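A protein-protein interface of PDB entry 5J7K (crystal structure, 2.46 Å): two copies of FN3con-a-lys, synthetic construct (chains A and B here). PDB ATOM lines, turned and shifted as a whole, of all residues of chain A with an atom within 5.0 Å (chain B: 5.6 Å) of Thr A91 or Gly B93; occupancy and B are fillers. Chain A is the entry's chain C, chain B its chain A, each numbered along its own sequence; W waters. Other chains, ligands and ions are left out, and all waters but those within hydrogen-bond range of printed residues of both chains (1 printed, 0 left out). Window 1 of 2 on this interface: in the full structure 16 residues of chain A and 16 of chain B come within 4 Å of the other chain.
A ring nitrogen (NE2) of His B94 lies within hydrogen-bond range of the side-chain hydroxyl (OG1) of Thr A91. The backbone carbonyl oxygen (O) of Ser A89 sits at hydrogen-bond distance from the backbone NH (N) of His B95, at 3.2 Å.
The side-chain hydroxyl (OG) of Ser B15 lies within hydrogen-bond range of the backbone carbonyl oxygen (O) of Gly B93, 3.4 Å away. A ring nitrogen (ND1) of His B94 lies close to a ring nitrogen (NE2) of His B95. The backbone NH (N) of Gly A63 is in hydrogen-bond range of the backbone carbonyl oxygen (O) of Gly A93, at 2.8 Å. The backbone NH of Tyr A66 is in hydrogen-bond range of the backbone carbonyl oxygen of Val A90 (2.6 Å).
Val A13 touches Thr B14. CB of Val A13 touches OG of Ser B15 (3.4 Å). O of His B94 touches C of Val A90, at 3.1 Å. His B95 touches Val A90. Thr A91 touches Gly B93 (O to CA, 3.0 Å). CA of Gly A93 touches O of Thr B91, 3.3 Å away.
Printed residues of chain B within 4 Å of Thr A91: Gly B93 and His B94. Of the printed residues of chain A, Gly B93 touches Thr A91 (3.0 Å). Of the printed residues of chain A, Thr B91 touches Gly A93. Printed residues of chain B within 4 Å of Ser A89: His B95. Of the printed residues of chain B, Gly A93 touches Thr B91. Of the printed residues of chain A, Thr B14 touches Val A13. Thr A64 touches none of the printed residues of chain B. Thr A92 touches none of the printed residues of chain B. The nearest residue of chain B that does not touch Thr A91 is His B95 (4.1 Å). The nearest printed residue of chain A that does not touch Gly B93 is Val A13 (4.01 Å). The nearest printed residue of chain A that does not touch His B95 is Thr A91 (4.1 Å).
Of the 10 printed residues of chain A, 5 touch a printed residue of chain B. Of the 9 printed residues of chain B, 6 touch a printed residue of chain A. Printed residues of chain B that touch a printed residue of chain A: Thr B14, Ser B15, Thr B91, Gly B93, His B94 and His B95. Hydrophobic or aromatic side chains of chain B within 4 Å of the printed part of chain A: His B94 and His B95. Among the printed residues, 8 pairs touch across the chains. Among the printed residues, no Asp or Glu carboxylate lies within 4 Å of a Lys or Arg side-chain nitrogen of the other chain.
Thr A91 touches Gly B93, and with the chains exchanged Gly A93 touches Thr B91. Of the 8 pairs that touch across the chains among the printed residues, 2 have their exchanged pair printed and touching as well.
Water W1 bridges a ring nitrogen (NE2) of His B94 (2.5 Å) and the side-chain hydroxyl of Thr A91 (2.5 Å).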
ATOM      1  N   VAL A  13      23.538 -25.432 -21.841  1.00  0.00           N
ATOM      2  CA  VAL A  13      24.636 -24.580 -21.399  1.00  0.00           C
ATOM      3  C   VAL A  13      24.216 -23.893 -20.110  1.00  0.00           C
ATOM      4  O   VAL A  13      23.151 -23.271 -20.051  1.00  0.00           O
ATOM      5  CB  VAL A  13      25.015 -23.532 -22.466  1.00  0.00           C
ATOM      6  CG1 VAL A  13      25.815 -22.375 -21.846  1.00  0.00           C
ATOM      7  CG2 VAL A  13      25.768 -24.175 -23.595  1.00  0.00           C
ATOM      8  N   GLY A  63      30.245 -16.946 -17.330  1.00  0.00           N
ATOM      9  CA  GLY A  63      30.423 -15.792 -18.198  1.00  0.00           C
ATOM     10  C   GLY A  63      31.718 -15.713 -18.974  1.00  0.00           C
ATOM     11  O   GLY A  63      32.169 -14.609 -19.300  1.00  0.00           O
ATOM     12  N   THR A  64      32.323 -16.852 -19.296  1.00  0.00           N
ATOM     13  CA  THR A  64      33.587 -16.882 -20.018  1.00  0.00           C
ATOM     14  C   THR A  64      33.460 -17.805 -21.223  1.00  0.00           C
ATOM     15  O   THR A  64      32.724 -18.796 -21.197  1.00  0.00           O
ATOM     16  CB  THR A  64      34.763 -17.300 -19.130  1.00  0.00           C
ATOM     17  OG1 THR A  64      35.988 -17.145 -19.859  1.00  0.00           O
ATOM     18  CG2 THR A  64      34.624 -18.732 -18.694  1.00  0.00           C
ATOM     19  N   GLU A  65      34.171 -17.453 -22.286  1.00  0.00           N
ATOM     20  CA  GLU A  65      34.178 -18.229 -23.516  1.00  0.00           C
ATOM     21  C   GLU A  65      35.123 -19.419 -23.396  1.00  0.00           C
ATOM     22  O   GLU A  65      36.308 -19.255 -23.083  1.00  0.00           O
ATOM     23  CB  GLU A  65      34.593 -17.305 -24.654  1.00  0.00           C
ATOM     24  CG  GLU A  65      33.589 -16.200 -24.849  1.00  0.00           C
ATOM     25  CD  GLU A  65      33.859 -15.369 -26.064  1.00  0.00           C
ATOM     26  OE1 GLU A  65      34.238 -14.206 -25.843  1.00  0.00           O
ATOM     27  OE2 GLU A  65      33.732 -15.855 -27.205  1.00  0.00           O
ATOM     28  N   TYR A  66      34.602 -20.606 -23.693  1.00  0.00           N
ATOM     29  CA  TYR A  66      35.320 -21.871 -23.646  1.00  0.00           C
ATOM     30  C   TYR A  66      35.300 -22.531 -25.018  1.00  0.00           C
ATOM     31  O   TYR A  66      34.439 -22.255 -25.858  1.00  0.00           O
ATOM     32  CB  TYR A  66      34.714 -22.868 -22.646  1.00  0.00           C
ATOM     33  CG  TYR A  66      34.970 -22.675 -21.164  1.00  0.00           C
ATOM     34  CD1 TYR A  66      36.164 -23.102 -20.591  1.00  0.00           C
ATOM     35  CD2 TYR A  66      33.981 -22.186 -20.319  1.00  0.00           C
ATOM     36  CE1 TYR A  66      36.394 -22.981 -19.229  1.00  0.00           C
ATOM     37  CE2 TYR A  66      34.199 -22.067 -18.954  1.00  0.00           C
ATOM     38  CZ  TYR A  66      35.409 -22.462 -18.416  1.00  0.00           C
ATOM     39  OH  TYR A  66      35.627 -22.341 -17.062  1.00  0.00           O
ATOM     40  N   SER A  89      32.477 -23.693 -29.663  1.00  0.00           N
ATOM     41  CA  SER A  89      32.776 -22.639 -28.704  1.00  0.00           C
ATOM     42  C   SER A  89      31.539 -22.356 -27.859  1.00  0.00           C
ATOM     43  O   SER A  89      30.431 -22.237 -28.392  1.00  0.00           O
ATOM     44  CB  SER A  89      33.255 -21.375 -29.419  1.00  0.00           C
ATOM     45  OG  SER A  89      32.339 -20.992 -30.425  1.00  0.00           O
ATOM     46  N   VAL A  90      31.733 -22.226 -26.549  1.00  0.00           N
ATOM     47  CA  VAL A  90      30.641 -22.065 -25.600  1.00  0.00           C
ATOM     48  C   VAL A  90      30.950 -20.901 -24.669  1.00  0.00           C
ATOM     49  O   VAL A  90      32.089 -20.735 -24.223  1.00  0.00           O
ATOM     50  CB  VAL A  90      30.414 -23.354 -24.786  1.00  0.00           C
ATOM     51  CG1 VAL A  90      29.274 -23.152 -23.841  1.00  0.00           C
ATOM     52  CG2 VAL A  90      30.152 -24.543 -25.710  1.00  0.00           C
ATOM     53  N   THR A  91      29.929 -20.099 -24.376  1.00  0.00           N
ATOM     54  CA  THR A  91      29.977 -19.057 -23.356  1.00  0.00           C
ATOM     55  C   THR A  91      28.951 -19.375 -22.284  1.00  0.00           C
ATOM     56  O   THR A  91      27.813 -19.729 -22.594  1.00  0.00           O
ATOM     57  CB  THR A  91      29.699 -17.674 -23.939  1.00  0.00           C
ATOM     58  OG1 THR A  91      30.695 -17.370 -24.919  1.00  0.00           O
ATOM     59  CG2 THR A  91      29.731 -16.608 -22.864  1.00  0.00           C
ATOM     60  N   THR A  92      29.378 -19.313 -21.034  1.00  0.00           N
ATOM     61  CA  THR A  92      28.535 -19.578 -19.879  1.00  0.00           C
ATOM     62  C   THR A  92      27.741 -18.326 -19.491  1.00  0.00           C
ATOM     63  O   THR A  92      27.970 -17.223 -20.000  1.00  0.00           O
ATOM     64  CB  THR A  92      29.382 -20.062 -18.709  1.00  0.00           C
ATOM     65  OG1 THR A  92      30.495 -19.180 -18.537  1.00  0.00           O
ATOM     66  CG2 THR A  92      29.910 -21.458 -18.999  1.00  0.00           C
ATOM     67  N   GLY A  93      26.787 -18.520 -18.571  1.00  0.00           N
ATOM     68  CA  GLY A  93      25.916 -17.452 -18.134  1.00  0.00           C
ATOM     69  C   GLY A  93      26.577 -16.490 -17.159  1.00  0.00           C
ATOM     70  O   GLY A  93      27.562 -16.802 -16.489  1.00  0.00           O
ATOM     71  N   THR B  14      20.155 -21.056 -18.236  1.00  0.00           N
ATOM     72  CA  THR B  14      20.451 -21.822 -19.439  1.00  0.00           C
ATOM     73  C   THR B  14      20.497 -20.860 -20.628  1.00  0.00           C
ATOM     74  O   THR B  14      20.383 -19.643 -20.475  1.00  0.00           O
ATOM     75  CB  THR B  14      19.445 -22.959 -19.652  1.00  0.00           C
ATOM     76  OG1 THR B  14      18.191 -22.427 -20.091  1.00  0.00           O
ATOM     77  CG2 THR B  14      19.242 -23.745 -18.361  1.00  0.00           C
ATOM     78  N   SER B  15      20.708 -21.422 -21.816  1.00  0.00           N
ATOM     79  CA  SER B  15      20.686 -20.618 -23.035  1.00  0.00           C
ATOM     80  C   SER B  15      19.315 -20.005 -23.302  1.00  0.00           C
ATOM     81  O   SER B  15      19.231 -18.915 -23.879  1.00  0.00           O
ATOM     82  CB  SER B  15      21.120 -21.473 -24.223  1.00  0.00           C
ATOM     83  OG  SER B  15      22.276 -22.233 -23.908  1.00  0.00           O
ATOM     84  N   PRO B  62      19.270 -17.128 -26.700  1.00  0.00           N
ATOM     85  CA  PRO B  62      20.652 -17.357 -26.257  1.00  0.00           C
ATOM     86  C   PRO B  62      21.492 -16.096 -26.378  1.00  0.00           C
ATOM     87  O   PRO B  62      21.275 -15.261 -27.252  1.00  0.00           O
ATOM     88  CB  PRO B  62      21.149 -18.452 -27.200  1.00  0.00           C
ATOM     89  CG  PRO B  62      19.917 -19.111 -27.687  1.00  0.00           C
ATOM     90  CD  PRO B  62      18.827 -18.114 -27.690  1.00  0.00           C
ATOM     91  N   GLY B  63      22.419 -15.943 -25.441  1.00  0.00           N
ATOM     92  CA  GLY B  63      23.391 -14.868 -25.495  1.00  0.00           C
ATOM     93  C   GLY B  63      22.789 -13.487 -25.351  1.00  0.00           C
ATOM     94  O   GLY B  63      23.253 -12.544 -26.004  1.00  0.00           O
ATOM     95  N   THR B  91      22.751 -12.567 -18.286  1.00  0.00           N
ATOM     96  CA  THR B  91      23.136 -12.841 -19.673  1.00  0.00           C
ATOM     97  C   THR B  91      23.247 -14.344 -19.874  1.00  0.00           C
ATOM     98  O   THR B  91      23.960 -15.018 -19.122  1.00  0.00           O
ATOM     99  CB  THR B  91      24.467 -12.176 -20.052  1.00  0.00           C
ATOM    100  OG1 THR B  91      24.321 -10.750 -20.029  1.00  0.00           O
ATOM    101  CG2 THR B  91      24.933 -12.607 -21.437  1.00  0.00           C
ATOM    102  N   THR B  92      22.564 -14.860 -20.898  1.00  0.00           N
ATOM    103  CA  THR B  92      22.539 -16.285 -21.208  1.00  0.00           C
ATOM    104  C   THR B  92      23.740 -16.699 -22.071  1.00  0.00           C
ATOM    105  O   THR B  92      24.438 -15.866 -22.658  1.00  0.00           O
ATOM    106  CB  THR B  92      21.235 -16.644 -21.918  1.00  0.00           C
ATOM    107  OG1 THR B  92      20.993 -15.701 -22.966  1.00  0.00           O
ATOM    108  CG2 THR B  92      20.067 -16.580 -20.945  1.00  0.00           C
ATOM    109  N   GLY B  93      23.987 -18.010 -22.118  1.00  0.00           N
ATOM    110  CA  GLY B  93      25.112 -18.559 -22.859  1.00  0.00           C
ATOM    111  C   GLY B  93      24.886 -18.927 -24.321  1.00  0.00           C
ATOM    112  O   GLY B  93      23.783 -19.251 -24.741  1.00  0.00           O
ATOM    113  N   HIS B  94      25.979 -18.873 -25.085  1.00  0.00           N
ATOM    114  CA  HIS B  94      26.067 -19.190 -26.522  1.00  0.00           C
ATOM    115  C   HIS B  94      27.433 -19.878 -26.753  1.00  0.00           C
ATOM    116  O   HIS B  94      28.248 -19.811 -25.841  1.00  0.00           O
ATOM    117  CB  HIS B  94      25.939 -17.912 -27.333  1.00  0.00           C
ATOM    118  CG  HIS B  94      27.194 -17.106 -27.329  1.00  0.00           C
ATOM    119  ND1 HIS B  94      27.955 -16.897 -28.458  1.00  0.00           N
ATOM    120  CD2 HIS B  94      27.832 -16.472 -26.319  1.00  0.00           C
ATOM    121  CE1 HIS B  94      29.015 -16.178 -28.138  1.00  0.00           C
ATOM    122  NE2 HIS B  94      28.963 -15.901 -26.847  1.00  0.00           N
ATOM    123  N   HIS B  95      27.750 -20.542 -27.879  1.00  0.00           N
ATOM    124  CA  HIS B  95      26.872 -21.065 -28.929  1.00  0.00           C
ATOM    125  C   HIS B  95      26.318 -22.428 -28.539  1.00  0.00           C
ATOM    126  O   HIS B  95      26.963 -23.183 -27.809  1.00  0.00           O
ATOM    127  CB  HIS B  95      27.623 -21.284 -30.258  1.00  0.00           C
ATOM    128  CG  HIS B  95      28.199 -20.052 -30.884  1.00  0.00           C
ATOM    129  ND1 HIS B  95      29.321 -20.095 -31.685  1.00  0.00           N
ATOM    130  CD2 HIS B  95      27.797 -18.760 -30.874  1.00  0.00           C
ATOM    131  CE1 HIS B  95      29.599 -18.880 -32.122  1.00  0.00           C
ATOM    132  NE2 HIS B  95      28.690 -18.050 -31.642  1.00  0.00           N
HETATM  133  O   HOH W   1      30.769 -14.893 -25.486  1.00  0.00           O
